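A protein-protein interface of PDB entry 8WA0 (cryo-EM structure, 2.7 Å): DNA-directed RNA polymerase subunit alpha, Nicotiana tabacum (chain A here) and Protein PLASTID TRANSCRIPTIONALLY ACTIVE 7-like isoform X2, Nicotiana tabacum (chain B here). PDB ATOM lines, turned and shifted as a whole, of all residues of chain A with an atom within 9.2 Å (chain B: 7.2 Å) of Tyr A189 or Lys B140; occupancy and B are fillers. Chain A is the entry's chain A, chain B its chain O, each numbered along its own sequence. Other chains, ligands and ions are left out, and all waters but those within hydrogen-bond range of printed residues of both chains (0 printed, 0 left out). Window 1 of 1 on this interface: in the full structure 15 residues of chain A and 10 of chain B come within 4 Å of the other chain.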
ATOM      1  N   ILE A  33     -18.381   8.486   7.812  1.00  0.00           N
ATOM      2  CA  ILE A  33     -17.417   7.716   8.582  1.00  0.00           C
ATOM      3  C   ILE A  33     -16.090   8.465   8.699  1.00  0.00           C
ATOM      4  O   ILE A  33     -15.791   9.320   7.870  1.00  0.00           O
ATOM      5  CB  ILE A  33     -17.221   6.312   7.962  1.00  0.00           C
ATOM      6  CG1 ILE A  33     -16.858   5.282   9.029  1.00  0.00           C
ATOM      7  CG2 ILE A  33     -16.198   6.334   6.832  1.00  0.00           C
ATOM      8  CD1 ILE A  33     -16.662   3.892   8.468  1.00  0.00           C
ATOM      9  N   LEU A  34     -15.315   8.189   9.744  1.00  0.00           N
ATOM     10  CA  LEU A  34     -14.001   8.812   9.902  1.00  0.00           C
ATOM     11  C   LEU A  34     -12.984   7.699  10.104  1.00  0.00           C
ATOM     12  O   LEU A  34     -13.325   6.669  10.648  1.00  0.00           O
ATOM     13  CB  LEU A  34     -13.989   9.794  11.069  1.00  0.00           C
ATOM     14  CG  LEU A  34     -12.799  10.751  11.195  1.00  0.00           C
ATOM     15  CD1 LEU A  34     -12.595  11.550   9.918  1.00  0.00           C
ATOM     16  CD2 LEU A  34     -12.980  11.678  12.386  1.00  0.00           C
ATOM     17  N   PRO A  36      -9.399   5.460  11.295  1.00  0.00           N
ATOM     18  CA  PRO A  36      -9.034   5.061  12.654  1.00  0.00           C
ATOM     19  C   PRO A  36      -8.531   6.166  13.539  1.00  0.00           C
ATOM     20  O   PRO A  36      -7.673   6.954  13.148  1.00  0.00           O
ATOM     21  CB  PRO A  36      -7.875   4.082  12.419  1.00  0.00           C
ATOM     22  CG  PRO A  36      -7.792   3.858  10.936  1.00  0.00           C
ATOM     23  CD  PRO A  36      -9.065   4.381  10.355  1.00  0.00           C
ATOM     24  N   LEU A  37      -9.059   6.203  14.754  1.00  0.00           N
ATOM     25  CA  LEU A  37      -8.690   7.238  15.688  1.00  0.00           C
ATOM     26  C   LEU A  37      -8.160   6.552  16.920  1.00  0.00           C
ATOM     27  O   LEU A  37      -8.566   5.435  17.234  1.00  0.00           O
ATOM     28  CB  LEU A  37      -9.927   8.047  16.071  1.00  0.00           C
ATOM     29  CG  LEU A  37     -10.660   8.861  15.009  1.00  0.00           C
ATOM     30  CD1 LEU A  37     -12.155   8.888  15.286  1.00  0.00           C
ATOM     31  CD2 LEU A  37     -10.093  10.266  14.939  1.00  0.00           C
ATOM     32  N   ILE A 186     -19.834   4.694  17.910  1.00  0.00           N
ATOM     33  CA  ILE A 186     -18.452   4.251  17.837  1.00  0.00           C
ATOM     34  C   ILE A 186     -18.272   2.753  17.653  1.00  0.00           C
ATOM     35  O   ILE A 186     -19.066   1.998  18.154  1.00  0.00           O
ATOM     36  CB  ILE A 186     -17.671   4.667  19.103  1.00  0.00           C
ATOM     37  CG1 ILE A 186     -17.846   6.152  19.390  1.00  0.00           C
ATOM     38  CG2 ILE A 186     -16.189   4.373  18.996  1.00  0.00           C
ATOM     39  CD1 ILE A 186     -17.114   6.600  20.626  1.00  0.00           C
ATOM     40  N   HIS A 187     -17.277   2.298  16.915  1.00  0.00           N
ATOM     41  CA  HIS A 187     -16.956   0.888  16.819  1.00  0.00           C
ATOM     42  C   HIS A 187     -15.516   0.842  17.175  1.00  0.00           C
ATOM     43  O   HIS A 187     -14.780   1.685  16.765  1.00  0.00           O
ATOM     44  CB  HIS A 187     -17.087   0.359  15.434  1.00  0.00           C
ATOM     45  CG  HIS A 187     -18.479   0.001  15.039  1.00  0.00           C
ATOM     46  ND1 HIS A 187     -18.752  -0.772  13.933  1.00  0.00           N
ATOM     47  CD2 HIS A 187     -19.676   0.321  15.580  1.00  0.00           C
ATOM     48  CE1 HIS A 187     -20.058  -0.919  13.814  1.00  0.00           C
ATOM     49  NE2 HIS A 187     -20.642  -0.262  14.799  1.00  0.00           N
ATOM     50  N   SER A 188     -15.098  -0.127  17.967  1.00  0.00           N
ATOM     51  CA  SER A 188     -13.695  -0.277  18.320  1.00  0.00           C
ATOM     52  C   SER A 188     -13.151  -1.585  17.876  1.00  0.00           C
ATOM     53  O   SER A 188     -13.736  -2.600  18.152  1.00  0.00           O
ATOM     54  CB  SER A 188     -13.513  -0.181  19.801  1.00  0.00           C
ATOM     55  OG  SER A 188     -12.157  -0.326  20.155  1.00  0.00           O
ATOM     56  N   TYR A 189     -12.142  -1.556  17.018  1.00  0.00           N
ATOM     57  CA  TYR A 189     -11.619  -2.777  16.442  1.00  0.00           C
ATOM     58  C   TYR A 189     -10.202  -2.871  16.849  1.00  0.00           C
ATOM     59  O   TYR A 189      -9.321  -2.440  16.133  1.00  0.00           O
ATOM     60  CB  TYR A 189     -11.640  -2.709  14.927  1.00  0.00           C
ATOM     61  CG  TYR A 189     -12.976  -2.881  14.268  1.00  0.00           C
ATOM     62  CD1 TYR A 189     -13.421  -4.132  13.894  1.00  0.00           C
ATOM     63  CD2 TYR A 189     -13.772  -1.789  13.977  1.00  0.00           C
ATOM     64  CE1 TYR A 189     -14.636  -4.298  13.272  1.00  0.00           C
ATOM     65  CE2 TYR A 189     -14.990  -1.943  13.354  1.00  0.00           C
ATOM     66  CZ  TYR A 189     -15.416  -3.202  13.004  1.00  0.00           C
ATOM     67  OH  TYR A 189     -16.631  -3.370  12.383  1.00  0.00           O
ATOM     68  N   GLY A 190      -9.966  -3.433  18.009  1.00  0.00           N
ATOM     69  CA  GLY A 190      -8.618  -3.526  18.500  1.00  0.00           C
ATOM     70  C   GLY A 190      -8.151  -4.949  18.629  1.00  0.00           C
ATOM     71  O   GLY A 190      -8.845  -5.787  19.191  1.00  0.00           O
ATOM     72  N   ASN A 191      -6.981  -5.237  18.092  1.00  0.00           N
ATOM     73  CA  ASN A 191      -6.435  -6.561  18.237  1.00  0.00           C
ATOM     74  C   ASN A 191      -4.941  -6.512  18.382  1.00  0.00           C
ATOM     75  O   ASN A 191      -4.281  -5.651  17.811  1.00  0.00           O
ATOM     76  CB  ASN A 191      -6.787  -7.389  17.031  1.00  0.00           C
ATOM     77  N   GLY A 192      -4.398  -7.458  19.125  1.00  0.00           N
ATOM     78  CA  GLY A 192      -2.979  -7.456  19.357  1.00  0.00           C
ATOM     79  C   GLY A 192      -2.479  -6.212  20.046  1.00  0.00           C
ATOM     80  O   GLY A 192      -2.946  -5.864  21.127  1.00  0.00           O
ATOM     81  N   ASN A 193      -1.502  -5.552  19.442  1.00  0.00           N
ATOM     82  CA  ASN A 193      -0.900  -4.365  20.039  1.00  0.00           C
ATOM     83  C   ASN A 193      -1.734  -3.102  20.275  1.00  0.00           C
ATOM     84  O   ASN A 193      -1.610  -2.482  21.328  1.00  0.00           O
ATOM     85  CB  ASN A 193       0.316  -3.975  19.199  1.00  0.00           C
ATOM     86  CG  ASN A 193      -0.047  -3.614  17.768  1.00  0.00           C
ATOM     87  OD1 ASN A 193      -1.047  -4.084  17.223  1.00  0.00           O
ATOM     88  ND2 ASN A 193       0.769  -2.770  17.152  1.00  0.00           N
ATOM     89  N   GLU A 194      -2.578  -2.704  19.329  1.00  0.00           N
ATOM     90  CA  GLU A 194      -3.287  -1.431  19.482  1.00  0.00           C
ATOM     91  C   GLU A 194      -4.741  -1.401  19.071  1.00  0.00           C
ATOM     92  O   GLU A 194      -5.213  -2.272  18.347  1.00  0.00           O
ATOM     93  CB  GLU A 194      -2.541  -0.314  18.762  1.00  0.00           C
ATOM     94  N   LYS A 195      -5.450  -0.382  19.534  1.00  0.00           N
ATOM     95  CA  LYS A 195      -6.855  -0.275  19.235  1.00  0.00           C
ATOM     96  C   LYS A 195      -7.138   0.889  18.314  1.00  0.00           C
ATOM     97  O   LYS A 195      -6.480   1.912  18.396  1.00  0.00           O
ATOM     98  CB  LYS A 195      -7.629  -0.126  20.532  1.00  0.00           C
ATOM     99  CG  LYS A 195      -7.072  -0.961  21.672  1.00  0.00           C
ATOM    100  CD  LYS A 195      -8.047  -1.032  22.831  1.00  0.00           C
ATOM    101  CE  LYS A 195      -9.315  -1.756  22.420  1.00  0.00           C
ATOM    102  NZ  LYS A 195     -10.305  -1.825  23.528  1.00  0.00           N
ATOM    103  N   GLN A 196      -8.095   0.726  17.415  1.00  0.00           N
ATOM    104  CA  GLN A 196      -8.448   1.767  16.484  1.00  0.00           C
ATOM    105  C   GLN A 196      -9.938   1.921  16.593  1.00  0.00           C
ATOM    106  O   GLN A 196     -10.623   0.971  16.923  1.00  0.00           O
ATOM    107  CB  GLN A 196      -8.127   1.317  15.077  1.00  0.00           C
ATOM    108  CG  GLN A 196      -6.730   0.774  14.879  1.00  0.00           C
ATOM    109  CD  GLN A 196      -6.533   0.244  13.481  1.00  0.00           C
ATOM    110  OE1 GLN A 196      -5.530  -0.399  13.183  1.00  0.00           O
ATOM    111  NE2 GLN A 196      -7.498   0.509  12.612  1.00  0.00           N
ATOM    112  N   GLU A 197     -10.453   3.108  16.318  1.00  0.00           N
ATOM    113  CA  GLU A 197     -11.873   3.344  16.421  1.00  0.00           C
ATOM    114  C   GLU A 197     -12.426   3.991  15.184  1.00  0.00           C
ATOM    115  O   GLU A 197     -11.680   4.561  14.417  1.00  0.00           O
ATOM    116  CB  GLU A 197     -12.150   4.245  17.602  1.00  0.00           C
ATOM    117  CG  GLU A 197     -11.780   3.664  18.952  1.00  0.00           C
ATOM    118  CD  GLU A 197     -11.878   4.687  20.062  1.00  0.00           C
ATOM    119  OE1 GLU A 197     -11.822   5.895  19.762  1.00  0.00           O
ATOM    120  OE2 GLU A 197     -12.003   4.287  21.237  1.00  0.00           O
ATOM    121  N   ILE A 198     -13.731   3.900  14.972  1.00  0.00           N
ATOM    122  CA  ILE A 198     -14.362   4.551  13.855  1.00  0.00           C
ATOM    123  C   ILE A 198     -15.542   5.380  14.344  1.00  0.00           C
ATOM    124  O   ILE A 198     -16.335   4.905  15.099  1.00  0.00           O
ATOM    125  CB  ILE A 198     -14.818   3.539  12.785  1.00  0.00           C
ATOM    126  N   LEU A 199     -15.675   6.614  13.905  1.00  0.00           N
ATOM    127  CA  LEU A 199     -16.794   7.413  14.273  1.00  0.00           C
ATOM    128  C   LEU A 199     -17.788   7.375  13.180  1.00  0.00           C
ATOM    129  O   LEU A 199     -17.409   7.439  12.054  1.00  0.00           O
ATOM    130  CB  LEU A 199     -16.362   8.845  14.524  1.00  0.00           C
ATOM    131  CG  LEU A 199     -17.379   9.927  14.840  1.00  0.00           C
ATOM    132  CD1 LEU A 199     -18.003   9.697  16.201  1.00  0.00           C
ATOM    133  CD2 LEU A 199     -16.664  11.256  14.797  1.00  0.00           C
ATOM    134  N   PHE A 200     -19.067   7.242  13.514  1.00  0.00           N
ATOM    135  CA  PHE A 200     -20.135   7.228  12.534  1.00  0.00           C
ATOM    136  C   PHE A 200     -21.071   8.363  12.864  1.00  0.00           C
ATOM    137  O   PHE A 200     -21.562   8.431  13.969  1.00  0.00           O
ATOM    138  CB  PHE A 200     -20.927   5.945  12.635  1.00  0.00           C
ATOM    139  CG  PHE A 200     -20.188   4.719  12.211  1.00  0.00           C
ATOM    140  CD1 PHE A 200     -19.422   4.008  13.114  1.00  0.00           C
ATOM    141  CD2 PHE A 200     -20.300   4.247  10.922  1.00  0.00           C
ATOM    142  CE1 PHE A 200     -18.754   2.868  12.729  1.00  0.00           C
ATOM    143  CE2 PHE A 200     -19.640   3.105  10.530  1.00  0.00           C
ATOM    144  CZ  PHE A 200     -18.864   2.414  11.435  1.00  0.00           C
ATOM    145  N   ASP B 137     -18.370  -7.954   7.959  1.00  0.00           N
ATOM    146  CA  ASP B 137     -18.150  -6.638   8.550  1.00  0.00           C
ATOM    147  C   ASP B 137     -17.509  -5.776   7.523  1.00  0.00           C
ATOM    148  O   ASP B 137     -16.340  -5.938   7.214  1.00  0.00           O
ATOM    149  CB  ASP B 137     -17.283  -6.671   9.792  1.00  0.00           C
ATOM    150  CG  ASP B 137     -17.985  -7.296  10.976  1.00  0.00           C
ATOM    151  OD1 ASP B 137     -19.172  -7.664  10.843  1.00  0.00           O
ATOM    152  OD2 ASP B 137     -17.351  -7.420  12.045  1.00  0.00           O
ATOM    153  N   PRO B 138     -18.258  -4.826   6.999  1.00  0.00           N
ATOM    154  CA  PRO B 138     -17.741  -4.019   5.927  1.00  0.00           C
ATOM    155  C   PRO B 138     -16.550  -3.226   6.340  1.00  0.00           C
ATOM    156  O   PRO B 138     -15.677  -3.070   5.514  1.00  0.00           O
ATOM    157  CB  PRO B 138     -18.914  -3.133   5.608  1.00  0.00           C
ATOM    158  CG  PRO B 138     -20.115  -3.860   6.072  1.00  0.00           C
ATOM    159  CD  PRO B 138     -19.632  -4.448   7.350  1.00  0.00           C
ATOM    160  N   PHE B 139     -16.490  -2.746   7.572  1.00  0.00           N
ATOM    161  CA  PHE B 139     -15.447  -1.832   8.020  1.00  0.00           C
ATOM    162  C   PHE B 139     -14.282  -2.325   8.872  1.00  0.00           C
ATOM    163  O   PHE B 139     -13.634  -1.537   9.510  1.00  0.00           O
ATOM    164  CB  PHE B 139     -16.120  -0.684   8.736  1.00  0.00           C
ATOM    165  CG  PHE B 139     -17.307  -0.125   8.025  1.00  0.00           C
ATOM    166  CD1 PHE B 139     -17.168   0.506   6.810  1.00  0.00           C
ATOM    167  CD2 PHE B 139     -18.556  -0.208   8.591  1.00  0.00           C
ATOM    168  CE1 PHE B 139     -18.264   1.024   6.160  1.00  0.00           C
ATOM    169  CE2 PHE B 139     -19.656   0.308   7.951  1.00  0.00           C
ATOM    170  CZ  PHE B 139     -19.511   0.927   6.733  1.00  0.00           C
ATOM    171  N   LYS B 140     -13.995  -3.606   8.867  1.00  0.00           N
ATOM    172  CA  LYS B 140     -12.941  -4.137   9.693  1.00  0.00           C
ATOM    173  C   LYS B 140     -11.654  -3.589   9.262  1.00  0.00           C
ATOM    174  O   LYS B 140     -11.372  -3.504   8.084  1.00  0.00           O
ATOM    175  CB  LYS B 140     -12.899  -5.646   9.686  1.00  0.00           C
ATOM    176  N   PRO B 141     -10.833  -3.238  10.220  1.00  0.00           N
ATOM    177  CA  PRO B 141      -9.598  -2.588   9.886  1.00  0.00           C
ATOM    178  C   PRO B 141      -8.649  -3.425   9.042  1.00  0.00           C
ATOM    179  O   PRO B 141      -8.051  -2.896   8.121  1.00  0.00           O
ATOM    180  CB  PRO B 141      -9.052  -2.275  11.247  1.00  0.00           C
ATOM    181  N   GLY B 142      -8.512  -4.705   9.332  1.00  0.00           N
ATOM    182  CA  GLY B 142      -7.607  -5.557   8.592  1.00  0.00           C
ATOM    183  C   GLY B 142      -7.676  -6.977   9.091  1.00  0.00           C
ATOM    184  O   GLY B 142      -8.502  -7.280   9.946  1.00  0.00           O
ATOM    185  N   PRO B 143      -6.826  -7.862   8.574  1.00  0.00           N
ATOM    186  CA  PRO B 143      -6.774  -9.237   9.081  1.00  0.00           C
ATOM    187  C   PRO B 143      -6.306  -9.287  10.509  1.00  0.00           C
ATOM    188  O   PRO B 143      -5.456  -8.492  10.900  1.00  0.00           O
ATOM    189  CB  PRO B 143      -5.725  -9.895   8.209  1.00  0.00           C
ATOM    190  CG  PRO B 143      -4.941  -8.782   7.594  1.00  0.00           C
ATOM    191  CD  PRO B 143      -5.902  -7.645   7.451  1.00  0.00           C
ATOM    192  N   TYR B 145      -8.110  -8.596  13.259  1.00  0.00           N
ATOM    193  CA  TYR B 145      -8.659  -7.504  14.066  1.00  0.00           C
ATOM    194  C   TYR B 145     -10.026  -7.890  14.623  1.00  0.00           C
ATOM    195  O   TYR B 145     -10.853  -8.429  13.902  1.00  0.00           O
ATOM    196  CB  TYR B 145      -8.722  -6.230  13.250  1.00  0.00           C
ATOM    197  CG  TYR B 145      -7.534  -5.344  13.472  1.00  0.00           C
ATOM    198  CD1 TYR B 145      -7.412  -4.609  14.633  1.00  0.00           C
ATOM    199  CD2 TYR B 145      -6.523  -5.257  12.532  1.00  0.00           C
ATOM    200  CE1 TYR B 145      -6.323  -3.798  14.856  1.00  0.00           C
ATOM    201  CE2 TYR B 145      -5.428  -4.448  12.744  1.00  0.00           C
ATOM    202  CZ  TYR B 145      -5.336  -3.723  13.910  1.00  0.00           C
ATOM    203  OH  TYR B 145      -4.252  -2.914  14.136  1.00  0.00           O
ATOM    204  N   LEU B 146     -10.275  -7.618  15.897  1.00  0.00           N
ATOM    205  CA  LEU B 146     -11.521  -8.060  16.524  1.00  0.00           C
ATOM    206  C   LEU B 146     -12.406  -6.966  17.084  1.00  0.00           C
ATOM    207  O   LEU B 146     -11.940  -6.118  17.832  1.00  0.00           O
ATOM    208  CB  LEU B 146     -11.173  -8.984  17.679  1.00  0.00           C
ATOM    209  CG  LEU B 146     -11.243 -10.483  17.421  1.00  0.00           C
ATOM    210  CD1 LEU B 146     -11.522 -11.264  18.693  1.00  0.00           C
ATOM    211  CD2 LEU B 146     -12.296 -10.753  16.368  1.00  0.00           C
ATOM    212  N   LYS B 147     -13.695  -7.011  16.767  1.00  0.00           N
ATOM    213  CA  LYS B 147     -14.619  -5.996  17.251  1.00  0.00           C
ATOM    214  C   LYS B 147     -14.958  -6.184  18.705  1.00  0.00           C
ATOM    215  O   LYS B 147     -15.143  -7.308  19.144  1.00  0.00           O
ATOM    216  CB  LYS B 147     -15.899  -5.991  16.432  1.00  0.00           C
ATOM    217  N   ASP B 148     -15.061  -5.097  19.454  1.00  0.00           N
ATOM    218  CA  ASP B 148     -15.358  -5.150  20.860  1.00  0.00           C
ATOM    219  C   ASP B 148     -16.804  -4.867  21.071  1.00  0.00           C
ATOM    220  O   ASP B 148     -17.192  -3.709  21.175  1.00  0.00           O
ATOM    221  CB  ASP B 148     -14.529  -4.126  21.591  1.00  0.00           C
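Hydrophobic or aromatic side chains of chain B within 4 Å of the printed part of chain A: Phe B139, Pro B141 and Tyr B145.
Printed residues of chain A that touch a printed residue of chain B: Ile A33, Ser A188, Tyr A189, Gly A190, Asn A191, Glu A194, Gln A196 and Phe A200.
Hydrophobic or aromatic side chains of chain A that line the printed part of chain B: Ile A33, Tyr A189 and Phe A200.
The backbone NH of Asp B148 is in hydrogen-bond range of the backbone carbonyl oxygen of Ser A188.
O of Leu B146 sits at hydrogen-bond distance from N of Gly A190, 3.3 Å away.
The side-chain amide oxygen of Gln A196 lies within hydrogen-bond range of the side-chain hydroxyl of Tyr B145, 3.0 Å away.
The backbone NH (N) of Tyr A189 sits at hydrogen-bond distance from the backbone carbonyl oxygen (O) of Gln A196, 2.9 Å away.
Printed residues of chain B within 4 Å of Ser A188: Leu B146, Lys B147 and Asp B148.
Tyr A189 touches just these residues of chain B: Lys B140 (3.96 Å), Tyr B145 (3.3 Å), Leu B146 (3.6 Å) and Lys B147 (3.8 Å).
Printed residues of chain B within 4 Å of Gly A190: Leu B146 (3.3 Å).
Of the printed residues of chain B, Glu A194 touches Tyr B145 (3.97 Å).
Printed residues of chain B within 4 Å of Phe A200: Phe B139.
Lys B140 touches one residue of chain A.
The nearest residue of chain A that does not touch Lys B140 is Gln A196 (6.7 Å).
The nearest printed residue of chain A that does not touch Tyr B145 is Gly A190 (4.1 Å).
Among the printed residues, merely in contact across the chains: Ile A33 with Phe B139, Ser A188 with Leu B146, Ser A188 with Lys B147, Tyr A189 with Lys B140, Tyr A189 with Tyr B145, Tyr A189 with Leu B146, Tyr A189 with Lys B147, Asn A191 with Tyr B145, Asn A191 with Leu B146, Glu A194 with Tyr B145, Gln A196 with Pro B141 and Phe A200 with Phe B139.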
